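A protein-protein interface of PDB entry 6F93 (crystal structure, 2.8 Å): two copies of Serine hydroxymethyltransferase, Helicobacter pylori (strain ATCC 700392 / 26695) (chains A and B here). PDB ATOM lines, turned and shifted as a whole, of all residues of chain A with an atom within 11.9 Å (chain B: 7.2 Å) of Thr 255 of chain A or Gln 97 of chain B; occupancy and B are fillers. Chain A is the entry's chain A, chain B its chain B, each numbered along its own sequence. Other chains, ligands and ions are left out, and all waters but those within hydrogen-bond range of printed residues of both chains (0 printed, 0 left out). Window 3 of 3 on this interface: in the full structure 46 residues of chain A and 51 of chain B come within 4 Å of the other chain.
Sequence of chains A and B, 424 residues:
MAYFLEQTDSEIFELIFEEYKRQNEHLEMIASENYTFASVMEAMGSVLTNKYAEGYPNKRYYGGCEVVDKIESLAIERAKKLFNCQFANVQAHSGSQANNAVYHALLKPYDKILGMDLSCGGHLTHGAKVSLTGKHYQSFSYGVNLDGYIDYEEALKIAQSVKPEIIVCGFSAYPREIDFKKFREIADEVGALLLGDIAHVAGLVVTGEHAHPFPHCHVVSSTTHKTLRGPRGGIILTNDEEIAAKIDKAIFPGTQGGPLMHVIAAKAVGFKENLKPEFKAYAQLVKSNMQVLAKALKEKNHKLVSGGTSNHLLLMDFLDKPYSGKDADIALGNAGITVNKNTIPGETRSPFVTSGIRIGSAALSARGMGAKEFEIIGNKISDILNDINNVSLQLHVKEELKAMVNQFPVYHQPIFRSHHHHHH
Of the printed residues of chain A, Gln 97 of chain B touches Thr 255.
No residue of chain B comes within 4 Å of Gly 254 of chain A.
No residue of chain A comes within 4 Å of Ala 92 of chain B.
No residue of chain A comes within 4 Å of His 93 of chain B.
Of the printed residues of chain A, Ser 94 of chain B touches Thr 255 (2.6 Å).
No residue of chain A comes within 4 Å of Gly 95 of chain B.
No residue of chain A comes within 4 Å of Ser 96 of chain B.
Ala 98 of chain B touches none of the printed residues of chain A.
No residue of chain A comes within 4 Å of Asn 99 of chain B.
No residue of chain A comes within 4 Å of Asn 100 of chain B.
No residue of chain A comes within 4 Å of Ile 251 of chain B.
No residue of chain A comes within 4 Å of Gly 254 of chain B.
No residue of chain A comes within 4 Å of Thr 255 of chain B.
Of the printed residues of chain B, Tyr 52 of chain A touches Arg 232.
Of the printed residues of chain B, Gly 258 of chain A touches Arg 232 (3.1 Å).
Of the printed residues of chain B, Gln 97 of chain A touches Gln 256 (3.8 Å).
The nearest residue of chain A that does not touch Gln 97 of chain B is Gly 254 of chain A (6.1 Å).
The nearest printed residue of chain B that does not touch Gln 256 of chain A is Ser 94 of chain B (4.2 Å).
N of His 93 of chain A is in hydrogen-bond range of OE1 of Gln 97 of chain A, 3.0 Å away.
The side-chain amide oxygen (OE1) of Gln 97 of chain B sits at hydrogen-bond distance from the backbone NH (N) of His 93 of chain B (2.5 Å).
The side-chain hydroxyl (OG) of Ser 94 of chain B lies close to the backbone NH (N) of Gln 97 of chain B (3.3 Å).
Among the printed residues, merely in contact across the chains: Tyr 52 of chain A with Arg 232 of chain B (3.4 Å), Thr 255 of chain A with Gln 97 of chain B (3.7 Å), Gln 97 of chain A with Gln 256 of chain B (3.8 Å), Ser 94 of chain A with Gln 256 of chain B (3.8 Å) and Gln 256 of chain A with Arg 232 of chain B (3.9 Å).
The backbone carbonyl oxygen of Thr 255 of chain A is in hydrogen-bond range of the side-chain hydroxyl of Ser 94 of chain B.
The backbone carbonyl oxygen of Gly 258 of chain A sits close to the guanidinium group of Arg 232 of chain B, at 3.2 Å.
Ser 94 of chain A touches Gln 256 of chain B, but with the chains exchanged Gln 256 of chain A does not touch Ser 94 of chain B (4.2 Å).
Gln 97 of chain A touches Gln 256 of chain B, but with the chains exchanged Gln 256 of chain A does not touch Gln 97 of chain B (6.5 Å).
Thr 255 of chain A touches Ser 94 of chain B, but with the chains exchanged Ser 94 of chain A does not touch Thr 255 of chain B (7.1 Å).
Thr 255 of chain A touches Gln 97 of chain B, but with the chains exchanged Gln 97 of chain A does not touch Thr 255 of chain B (6.8 Å).
Positions printed for both chains: 91, 92, 93, 94, 97, 101, 250, 251, 254, 255 and 256.
Of the 7 pairs that touch across the chains among the printed residues, none has its exchanged pair printed and touching as well.
Of the 22 printed residues of chain B, 4 touch a printed residue of chain A.
Among the printed residues, 7 pairs touch across the chains.
Among the printed residues, no Asp or Glu carboxylate lies within 4 Å of a Lys or Arg side-chain nitrogen of the other chain.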
ATOM      1  N   TYR A  52      44.400   1.758  31.366  1.00  0.00           N
ATOM      2  CA  TYR A  52      43.038   1.507  31.827  1.00  0.00           C
ATOM      3  C   TYR A  52      42.946   1.634  33.349  1.00  0.00           C
ATOM      4  O   TYR A  52      43.611   0.907  34.093  1.00  0.00           O
ATOM      5  CB  TYR A  52      42.564   0.121  31.383  1.00  0.00           C
ATOM      6  CG  TYR A  52      42.099   0.039  29.945  1.00  0.00           C
ATOM      7  CD1 TYR A  52      40.974  -0.719  29.604  1.00  0.00           C
ATOM      8  CD2 TYR A  52      42.769   0.724  28.930  1.00  0.00           C
ATOM      9  CE1 TYR A  52      40.541  -0.802  28.294  1.00  0.00           C
ATOM     10  CE2 TYR A  52      42.347   0.647  27.617  1.00  0.00           C
ATOM     11  CZ  TYR A  52      41.231  -0.117  27.307  1.00  0.00           C
ATOM     12  OH  TYR A  52      40.803  -0.196  26.005  1.00  0.00           O
ATOM     13  N   ASN A  89      33.448  13.974  42.649  1.00  0.00           N
ATOM     14  CA  ASN A  89      33.408  12.953  41.609  1.00  0.00           C
ATOM     15  C   ASN A  89      33.802  13.643  40.311  1.00  0.00           C
ATOM     16  O   ASN A  89      33.036  14.449  39.773  1.00  0.00           O
ATOM     17  CB  ASN A  89      32.019  12.317  41.524  1.00  0.00           C
ATOM     18  CG  ASN A  89      31.927  11.244  40.453  1.00  0.00           C
ATOM     19  OD1 ASN A  89      31.912  11.546  39.256  1.00  0.00           O
ATOM     20  ND2 ASN A  89      31.851   9.984  40.879  1.00  0.00           N
ATOM     21  N   GLN A  91      34.379  12.276  37.360  1.00  0.00           N
ATOM     22  CA  GLN A  91      34.214  11.372  36.231  1.00  0.00           C
ATOM     23  C   GLN A  91      33.075  11.751  35.295  1.00  0.00           C
ATOM     24  O   GLN A  91      32.958  11.145  34.228  1.00  0.00           O
ATOM     25  CB  GLN A  91      34.021   9.935  36.727  1.00  0.00           C
ATOM     26  CG  GLN A  91      35.322   9.312  37.193  1.00  0.00           C
ATOM     27  CD  GLN A  91      35.298   7.800  37.187  1.00  0.00           C
ATOM     28  OE1 GLN A  91      34.662   7.171  38.037  1.00  0.00           O
ATOM     29  NE2 GLN A  91      35.998   7.203  36.226  1.00  0.00           N
ATOM     30  N   ALA A  92      32.253  12.735  35.647  1.00  0.00           N
ATOM     31  CA  ALA A  92      31.199  13.180  34.747  1.00  0.00           C
ATOM     32  C   ALA A  92      31.792  13.659  33.425  1.00  0.00           C
ATOM     33  O   ALA A  92      32.812  14.354  33.398  1.00  0.00           O
ATOM     34  CB  ALA A  92      30.382  14.297  35.400  1.00  0.00           C
ATOM     35  N   HIS A  93      31.149  13.272  32.321  1.00  0.00           N
ATOM     36  CA  HIS A  93      31.632  13.578  30.977  1.00  0.00           C
ATOM     37  C   HIS A  93      31.179  14.938  30.469  1.00  0.00           C
ATOM     38  O   HIS A  93      31.654  15.379  29.418  1.00  0.00           O
ATOM     39  CB  HIS A  93      31.155  12.513  29.985  1.00  0.00           C
ATOM     40  CG  HIS A  93      32.103  11.368  29.804  1.00  0.00           C
ATOM     41  ND1 HIS A  93      33.108  11.376  28.861  1.00  0.00           N
ATOM     42  CD2 HIS A  93      32.179  10.166  30.424  1.00  0.00           C
ATOM     43  CE1 HIS A  93      33.770  10.233  28.915  1.00  0.00           C
ATOM     44  NE2 HIS A  93      33.226   9.482  29.855  1.00  0.00           N
ATOM     45  N   SER A  94      30.278  15.606  31.179  1.00  0.00           N
ATOM     46  CA  SER A  94      29.647  16.813  30.674  1.00  0.00           C
ATOM     47  C   SER A  94      28.992  17.548  31.833  1.00  0.00           C
ATOM     48  O   SER A  94      28.772  16.982  32.903  1.00  0.00           O
ATOM     49  CB  SER A  94      28.612  16.476  29.596  1.00  0.00           C
ATOM     50  OG  SER A  94      27.582  17.446  29.562  1.00  0.00           O
ATOM     51  N   GLN A  97      25.487  15.716  32.165  1.00  0.00           N
ATOM     52  CA  GLN A  97      25.530  14.488  32.952  1.00  0.00           C
ATOM     53  C   GLN A  97      25.621  14.794  34.439  1.00  0.00           C
ATOM     54  O   GLN A  97      24.942  14.153  35.251  1.00  0.00           O
ATOM     55  CB  GLN A  97      26.716  13.621  32.537  1.00  0.00           C
ATOM     56  CG  GLN A  97      26.542  12.851  31.262  1.00  0.00           C
ATOM     57  CD  GLN A  97      27.804  12.107  30.890  1.00  0.00           C
ATOM     58  OE1 GLN A  97      28.588  11.717  31.766  1.00  0.00           O
ATOM     59  NE2 GLN A  97      28.013  11.900  29.589  1.00  0.00           N
ATOM     60  N   ALA A 101      23.170  13.285  36.687  1.00  0.00           N
ATOM     61  CA  ALA A 101      23.631  12.280  37.641  1.00  0.00           C
ATOM     62  C   ALA A 101      23.201  12.625  39.061  1.00  0.00           C
ATOM     63  O   ALA A 101      22.900  11.729  39.858  1.00  0.00           O
ATOM     64  CB  ALA A 101      25.149  12.124  37.572  1.00  0.00           C
ATOM     65  N   ASP A 248      28.654   8.378  43.463  1.00  0.00           N
ATOM     66  CA  ASP A 248      29.614   7.432  42.903  1.00  0.00           C
ATOM     67  C   ASP A 248      28.918   6.274  42.190  1.00  0.00           C
ATOM     68  O   ASP A 248      29.381   5.825  41.134  1.00  0.00           O
ATOM     69  CB  ASP A 248      30.540   6.912  44.001  1.00  0.00           C
ATOM     70  CG  ASP A 248      31.504   7.971  44.503  1.00  0.00           C
ATOM     71  OD1 ASP A 248      31.899   8.847  43.701  1.00  0.00           O
ATOM     72  OD2 ASP A 248      31.875   7.923  45.699  1.00  0.00           O
ATOM     73  N   LYS A 249      27.807   5.771  42.748  1.00  0.00           N
ATOM     74  CA  LYS A 249      27.083   4.677  42.098  1.00  0.00           C
ATOM     75  C   LYS A 249      26.214   5.154  40.944  1.00  0.00           C
ATOM     76  O   LYS A 249      25.929   4.373  40.030  1.00  0.00           O
ATOM     77  CB  LYS A 249      26.197   3.915  43.093  1.00  0.00           C
ATOM     78  CG  LYS A 249      26.923   2.990  44.069  1.00  0.00           C
ATOM     79  CD  LYS A 249      27.329   3.706  45.334  1.00  0.00           C
ATOM     80  CE  LYS A 249      28.707   3.287  45.824  1.00  0.00           C
ATOM     81  NZ  LYS A 249      29.264   4.242  46.831  1.00  0.00           N
ATOM     82  N   ALA A 250      25.762   6.410  40.974  1.00  0.00           N
ATOM     83  CA  ALA A 250      24.943   6.920  39.881  1.00  0.00           C
ATOM     84  C   ALA A 250      25.780   7.166  38.633  1.00  0.00           C
ATOM     85  O   ALA A 250      25.350   6.848  37.517  1.00  0.00           O
ATOM     86  CB  ALA A 250      24.226   8.201  40.307  1.00  0.00           C
ATOM     87  N   ILE A 251      26.974   7.739  38.800  1.00  0.00           N
ATOM     88  CA  ILE A 251      27.883   7.900  37.672  1.00  0.00           C
ATOM     89  C   ILE A 251      28.240   6.543  37.076  1.00  0.00           C
ATOM     90  O   ILE A 251      28.422   6.422  35.859  1.00  0.00           O
ATOM     91  CB  ILE A 251      29.126   8.697  38.121  1.00  0.00           C
ATOM     92  CG1 ILE A 251      28.869  10.201  37.971  1.00  0.00           C
ATOM     93  CG2 ILE A 251      30.387   8.261  37.361  1.00  0.00           C
ATOM     94  CD1 ILE A 251      28.787  10.658  36.536  1.00  0.00           C
ATOM     95  N   PHE A 252      28.284   5.493  37.917  1.00  0.00           N
ATOM     96  CA  PHE A 252      28.641   4.093  37.663  1.00  0.00           C
ATOM     97  C   PHE A 252      29.649   3.926  36.517  1.00  0.00           C
ATOM     98  O   PHE A 252      30.853   4.031  36.789  1.00  0.00           O
ATOM     99  CB  PHE A 252      27.374   3.244  37.477  1.00  0.00           C
ATOM    100  N   PRO A 253      29.263   3.663  35.220  1.00  0.00           N
ATOM    101  CA  PRO A 253      30.313   3.230  34.288  1.00  0.00           C
ATOM    102  C   PRO A 253      31.007   4.355  33.525  1.00  0.00           C
ATOM    103  O   PRO A 253      32.237   4.356  33.399  1.00  0.00           O
ATOM    104  CB  PRO A 253      29.554   2.299  33.330  1.00  0.00           C
ATOM    105  CG  PRO A 253      28.111   2.801  33.354  1.00  0.00           C
ATOM    106  CD  PRO A 253      27.992   3.820  34.474  1.00  0.00           C
ATOM    107  N   GLY A 254      30.238   5.327  33.034  1.00  0.00           N
ATOM    108  CA  GLY A 254      30.660   6.052  31.855  1.00  0.00           C
ATOM    109  C   GLY A 254      30.523   5.226  30.598  1.00  0.00           C
ATOM    110  O   GLY A 254      30.988   5.647  29.534  1.00  0.00           O
ATOM    111  N   THR A 255      29.869   4.064  30.708  1.00  0.00           N
ATOM    112  CA  THR A 255      29.801   3.017  29.693  1.00  0.00           C
ATOM    113  C   THR A 255      31.145   2.804  29.005  1.00  0.00           C
ATOM    114  O   THR A 255      31.294   3.102  27.816  1.00  0.00           O
ATOM    115  CB  THR A 255      28.698   3.321  28.671  1.00  0.00           C
ATOM    116  OG1 THR A 255      29.067   4.451  27.868  1.00  0.00           O
ATOM    117  CG2 THR A 255      27.365   3.580  29.384  1.00  0.00           C
ATOM    118  N   GLN A 256      32.118   2.283  29.751  1.00  0.00           N
ATOM    119  CA  GLN A 256      33.432   1.929  29.233  1.00  0.00           C
ATOM    120  C   GLN A 256      34.203   1.203  30.325  1.00  0.00           C
ATOM    121  O   GLN A 256      34.171   1.615  31.488  1.00  0.00           O
ATOM    122  CB  GLN A 256      34.216   3.167  28.770  1.00  0.00           C
ATOM    123  N   GLY A 257      34.880   0.120  29.947  1.00  0.00           N
ATOM    124  CA  GLY A 257      35.800  -0.528  30.862  1.00  0.00           C
ATOM    125  C   GLY A 257      37.001   0.316  31.216  1.00  0.00           C
ATOM    126  O   GLY A 257      37.747  -0.040  32.135  1.00  0.00           O
ATOM    127  N   GLY A 258      37.198   1.424  30.516  1.00  0.00           N
ATOM    128  CA  GLY A 258      38.303   2.299  30.793  1.00  0.00           C
ATOM    129  C   GLY A 258      37.870   3.662  31.281  1.00  0.00           C
ATOM    130  O   GLY A 258      37.115   4.385  30.621  1.00  0.00           O
ATOM    131  N   PRO A 259      38.333   4.032  32.468  1.00  0.00           N
ATOM    132  CA  PRO A 259      38.286   5.446  32.854  1.00  0.00           C
ATOM    133  C   PRO A 259      39.342   6.199  32.057  1.00  0.00           C
ATOM    134  O   PRO A 259      40.509   5.798  32.026  1.00  0.00           O
ATOM    135  CB  PRO A 259      38.601   5.423  34.358  1.00  0.00           C
ATOM    136  CG  PRO A 259      38.639   3.952  34.755  1.00  0.00           C
ATOM    137  CD  PRO A 259      38.960   3.199  33.504  1.00  0.00           C
ATOM    138  N   LEU A 260      38.924   7.274  31.387  1.00  0.00           N
ATOM    139  CA  LEU A 260      39.817   7.963  30.453  1.00  0.00           C
ATOM    140  C   LEU A 260      40.793   8.835  31.240  1.00  0.00           C
ATOM    141  O   LEU A 260      40.475   9.963  31.632  1.00  0.00           O
ATOM    142  CB  LEU A 260      39.021   8.740  29.407  1.00  0.00           C
ATOM    143  CG  LEU A 260      38.150   7.857  28.488  1.00  0.00           C
ATOM    144  CD1 LEU A 260      36.816   7.403  29.085  1.00  0.00           C
ATOM    145  CD2 LEU A 260      37.872   8.537  27.174  1.00  0.00           C
ATOM    146  N   GLN B  91      30.131   9.236  16.210  1.00  0.00           N
ATOM    147  CA  GLN B  91      29.873  10.010  17.419  1.00  0.00           C
ATOM    148  C   GLN B  91      29.809   9.169  18.692  1.00  0.00           C
ATOM    149  O   GLN B  91      29.623   9.734  19.776  1.00  0.00           O
ATOM    150  CB  GLN B  91      28.577  10.811  17.260  1.00  0.00           C
ATOM    151  CG  GLN B  91      28.721  12.019  16.341  1.00  0.00           C
ATOM    152  CD  GLN B  91      27.385  12.622  15.950  1.00  0.00           C
ATOM    153  OE1 GLN B  91      26.331  12.188  16.427  1.00  0.00           O
ATOM    154  NE2 GLN B  91      27.419  13.633  15.080  1.00  0.00           N
ATOM    155  N   ALA B  92      29.976   7.854  18.605  1.00  0.00           N
ATOM    156  CA  ALA B  92      29.933   7.027  19.805  1.00  0.00           C
ATOM    157  C   ALA B  92      31.211   7.195  20.621  1.00  0.00           C
ATOM    158  O   ALA B  92      32.313   7.263  20.072  1.00  0.00           O
ATOM    159  CB  ALA B  92      29.727   5.560  19.429  1.00  0.00           C
ATOM    160  N   HIS B  93      31.060   7.257  21.948  1.00  0.00           N
ATOM    161  CA  HIS B  93      32.193   7.463  22.848  1.00  0.00           C
ATOM    162  C   HIS B  93      32.823   6.164  23.339  1.00  0.00           C
ATOM    163  O   HIS B  93      33.862   6.216  24.006  1.00  0.00           O
ATOM    164  CB  HIS B  93      31.774   8.296  24.067  1.00  0.00           C
ATOM    165  CG  HIS B  93      31.259   9.660  23.722  1.00  0.00           C
ATOM    166  ND1 HIS B  93      32.065  10.657  23.215  1.00  0.00           N
ATOM    167  CD2 HIS B  93      30.016  10.192  23.814  1.00  0.00           C
ATOM    168  CE1 HIS B  93      31.342  11.744  23.011  1.00  0.00           C
ATOM    169  NE2 HIS B  93      30.096  11.489  23.367  1.00  0.00           N
ATOM    170  N   SER B  94      32.230   5.014  23.033  1.00  0.00           N
ATOM    171  CA  SER B  94      32.786   3.734  23.448  1.00  0.00           C
ATOM    172  C   SER B  94      32.136   2.634  22.628  1.00  0.00           C
ATOM    173  O   SER B  94      31.046   2.807  22.079  1.00  0.00           O
ATOM    174  CB  SER B  94      32.568   3.479  24.941  1.00  0.00           C
ATOM    175  OG  SER B  94      31.224   3.752  25.303  1.00  0.00           O
ATOM    176  N   GLY B  95      32.819   1.491  22.555  1.00  0.00           N
ATOM    177  CA  GLY B  95      32.229   0.344  21.895  1.00  0.00           C
ATOM    178  C   GLY B  95      30.921  -0.090  22.524  1.00  0.00           C
ATOM    179  O   GLY B  95      30.025  -0.575  21.829  1.00  0.00           O
ATOM    180  N   SER B  96      30.786   0.082  23.839  1.00  0.00           N
ATOM    181  CA  SER B  96      29.551  -0.303  24.517  1.00  0.00           C
ATOM    182  C   SER B  96      28.422   0.666  24.195  1.00  0.00           C
ATOM    183  O   SER B  96      27.289   0.241  23.935  1.00  0.00           O
ATOM    184  CB  SER B  96      29.787  -0.375  26.027  1.00  0.00           C
ATOM    185  OG  SER B  96      31.074  -0.890  26.321  1.00  0.00           O
ATOM    186  N   GLN B  97      28.707   1.970  24.218  1.00  0.00           N
ATOM    187  CA  GLN B  97      27.691   2.957  23.878  1.00  0.00           C
ATOM    188  C   GLN B  97      27.298   2.881  22.407  1.00  0.00           C
ATOM    189  O   GLN B  97      26.192   3.296  22.046  1.00  0.00           O
ATOM    190  CB  GLN B  97      28.193   4.357  24.240  1.00  0.00           C
ATOM    191  CG  GLN B  97      27.225   5.487  23.926  1.00  0.00           C
ATOM    192  CD  GLN B  97      27.935   6.757  23.498  1.00  0.00           C
ATOM    193  OE1 GLN B  97      29.157   6.840  23.555  1.00  0.00           O
ATOM    194  NE2 GLN B  97      27.167   7.756  23.074  1.00  0.00           N
ATOM    195  N   ALA B  98      28.171   2.338  21.554  1.00  0.00           N
ATOM    196  CA  ALA B  98      27.792   2.101  20.167  1.00  0.00           C
ATOM    197  C   ALA B  98      26.803   0.947  20.059  1.00  0.00           C
ATOM    198  O   ALA B  98      25.842   1.015  19.285  1.00  0.00           O
ATOM    199  CB  ALA B  98      29.035   1.830  19.321  1.00  0.00           C
ATOM    200  N   ASN B  99      27.025  -0.124  20.821  1.00  0.00           N
ATOM    201  CA  ASN B  99      26.063  -1.221  20.857  1.00  0.00           C
ATOM    202  C   ASN B  99      24.705  -0.743  21.360  1.00  0.00           C
ATOM    203  O   ASN B  99      23.666  -1.025  20.749  1.00  0.00           O
ATOM    204  CB  ASN B  99      26.595  -2.349  21.737  1.00  0.00           C
ATOM    205  CG  ASN B  99      27.728  -3.104  21.087  1.00  0.00           C
ATOM    206  OD1 ASN B  99      27.706  -3.356  19.889  1.00  0.00           O
ATOM    207  ND2 ASN B  99      28.734  -3.462  21.876  1.00  0.00           N
ATOM    208  N   ASN B 100      24.696  -0.009  22.480  1.00  0.00           N
ATOM    209  CA  ASN B 100      23.435   0.457  23.044  1.00  0.00           C
ATOM    210  C   ASN B 100      22.719   1.422  22.106  1.00  0.00           C
ATOM    211  O   ASN B 100      21.483   1.434  22.054  1.00  0.00           O
ATOM    212  CB  ASN B 100      23.677   1.107  24.410  1.00  0.00           C
ATOM    213  CG  ASN B 100      24.119   0.103  25.467  1.00  0.00           C
ATOM    214  OD1 ASN B 100      23.749  -1.071  25.419  1.00  0.00           O
ATOM    215  ND2 ASN B 100      24.910   0.566  26.432  1.00  0.00           N
ATOM    216  N   ALA B 101      23.470   2.230  21.353  1.00  0.00           N
ATOM    217  CA  ALA B 101      22.838   3.115  20.382  1.00  0.00           C
ATOM    218  C   ALA B 101      22.167   2.326  19.262  1.00  0.00           C
ATOM    219  O   ALA B 101      21.146   2.765  18.719  1.00  0.00           O
ATOM    220  CB  ALA B 101      23.866   4.096  19.817  1.00  0.00           C
ATOM    221  N   VAL B 102      22.715   1.160  18.914  1.00  0.00           N
ATOM    222  CA  VAL B 102      22.082   0.308  17.911  1.00  0.00           C
ATOM    223  C   VAL B 102      20.800  -0.302  18.465  1.00  0.00           C
ATOM    224  O   VAL B 102      19.763  -0.330  17.786  1.00  0.00           O
ATOM    225  CB  VAL B 102      23.062  -0.779  17.435  1.00  0.00           C
ATOM    226  CG1 VAL B 102      22.351  -1.774  16.530  1.00  0.00           C
ATOM    227  CG2 VAL B 102      24.243  -0.143  16.722  1.00  0.00           C
ATOM    228  N   TYR B 103      20.855  -0.806  19.704  1.00  0.00           N
ATOM    229  CA  TYR B 103      19.663  -1.370  20.331  1.00  0.00           C
ATOM    230  C   TYR B 103      18.553  -0.330  20.453  1.00  0.00           C
ATOM    231  O   TYR B 103      17.386  -0.619  20.170  1.00  0.00           O
ATOM    232  CB  TYR B 103      19.994  -1.922  21.718  1.00  0.00           C
ATOM    233  CG  TYR B 103      21.072  -2.983  21.796  1.00  0.00           C
ATOM    234  CD1 TYR B 103      21.275  -3.897  20.768  1.00  0.00           C
ATOM    235  CD2 TYR B 103      21.875  -3.079  22.927  1.00  0.00           C
ATOM    236  CE1 TYR B 103      22.268  -4.874  20.868  1.00  0.00           C
ATOM    237  CE2 TYR B 103      22.862  -4.038  23.034  1.00  0.00           C
ATOM    238  CZ  TYR B 103      23.060  -4.930  22.010  1.00  0.00           C
ATOM    239  OH  TYR B 103      24.056  -5.869  22.149  1.00  0.00           O
ATOM    240  N   ARG B 232      40.082   6.242  21.906  1.00  0.00           N
ATOM    241  CA  ARG B 232      39.029   5.462  22.532  1.00  0.00           C
ATOM    242  C   ARG B 232      37.670   6.043  22.184  1.00  0.00           C
ATOM    243  O   ARG B 232      37.433   7.249  22.323  1.00  0.00           O
ATOM    244  CB  ARG B 232      39.236   5.394  24.041  1.00  0.00           C
ATOM    245  CG  ARG B 232      40.648   4.968  24.410  1.00  0.00           C
ATOM    246  CD  ARG B 232      40.722   4.646  25.867  1.00  0.00           C
ATOM    247  NE  ARG B 232      39.421   4.171  26.317  1.00  0.00           N
ATOM    248  CZ  ARG B 232      39.213   3.535  27.458  1.00  0.00           C
ATOM    249  NH1 ARG B 232      37.987   3.144  27.776  1.00  0.00           N
ATOM    250  NH2 ARG B 232      40.231   3.281  28.266  1.00  0.00           N
ATOM    251  N   GLY B 233      36.774   5.168  21.724  1.00  0.00           N
ATOM    252  CA  GLY B 233      35.497   5.578  21.229  1.00  0.00           C
ATOM    253  C   GLY B 233      34.869   4.422  20.405  1.00  0.00           C
ATOM    254  O   GLY B 233      35.430   3.345  20.346  1.00  0.00           O
ATOM    255  N   GLY B 234      33.732   4.764  19.810  1.00  0.00           N
ATOM    256  CA  GLY B 234      32.953   3.748  19.095  1.00  0.00           C
ATOM    257  C   GLY B 234      32.617   4.191  17.680  1.00  0.00           C
ATOM    258  O   GLY B 234      32.763   5.356  17.303  1.00  0.00           O
ATOM    259  N   ILE B 236      29.652   2.945  14.465  1.00  0.00           N
ATOM    260  CA  ILE B 236      28.533   2.145  13.976  1.00  0.00           C
ATOM    261  C   ILE B 236      28.487   2.237  12.456  1.00  0.00           C
ATOM    262  O   ILE B 236      28.487   3.338  11.895  1.00  0.00           O
ATOM    263  CB  ILE B 236      27.201   2.603  14.595  1.00  0.00           C
ATOM    264  CG1 ILE B 236      27.312   2.620  16.122  1.00  0.00           C
ATOM    265  CG2 ILE B 236      26.066   1.707  14.138  1.00  0.00           C
ATOM    266  CD1 ILE B 236      26.404   3.622  16.793  1.00  0.00           C
ATOM    267  N   ALA B 250      19.584   8.408  17.190  1.00  0.00           N
ATOM    268  CA  ALA B 250      19.901   7.850  18.502  1.00  0.00           C
ATOM    269  C   ALA B 250      21.185   8.448  19.061  1.00  0.00           C
ATOM    270  O   ALA B 250      21.378   8.476  20.283  1.00  0.00           O
ATOM    271  CB  ALA B 250      20.009   6.327  18.420  1.00  0.00           C
ATOM    272  N   ILE B 251      22.072   8.924  18.185  1.00  0.00           N
ATOM    273  CA  ILE B 251      23.247   9.659  18.638  1.00  0.00           C
ATOM    274  C   ILE B 251      22.888  11.109  18.942  1.00  0.00           C
ATOM    275  O   ILE B 251      23.534  11.745  19.782  1.00  0.00           O
ATOM    276  CB  ILE B 251      24.376   9.569  17.598  1.00  0.00           C
ATOM    277  N   GLY B 254      21.893  11.008  22.686  1.00  0.00           N
ATOM    278  CA  GLY B 254      23.054  10.623  23.465  1.00  0.00           C
ATOM    279  C   GLY B 254      24.313  11.365  23.064  1.00  0.00           C
ATOM    280  O   GLY B 254      25.425  10.863  23.264  1.00  0.00           O
ATOM    281  N   THR B 255      24.144  12.565  22.496  1.00  0.00           N
ATOM    282  CA  THR B 255      25.291  13.360  22.060  1.00  0.00           C
ATOM    283  C   THR B 255      26.183  13.736  23.238  1.00  0.00           C
ATOM    284  O   THR B 255      27.413  13.785  23.105  1.00  0.00           O
ATOM    285  CB  THR B 255      24.814  14.613  21.323  1.00  0.00           C
ATOM    286  N   GLN B 256      25.577  14.016  24.396  1.00  0.00           N
ATOM    287  CA  GLN B 256      26.296  14.224  25.656  1.00  0.00           C
ATOM    288  C   GLN B 256      27.219  15.443  25.592  1.00  0.00           C
ATOM    289  O   GLN B 256      28.404  15.372  25.925  1.00  0.00           O
ATOM    290  CB  GLN B 256      27.074  12.967  26.057  1.00  0.00           C
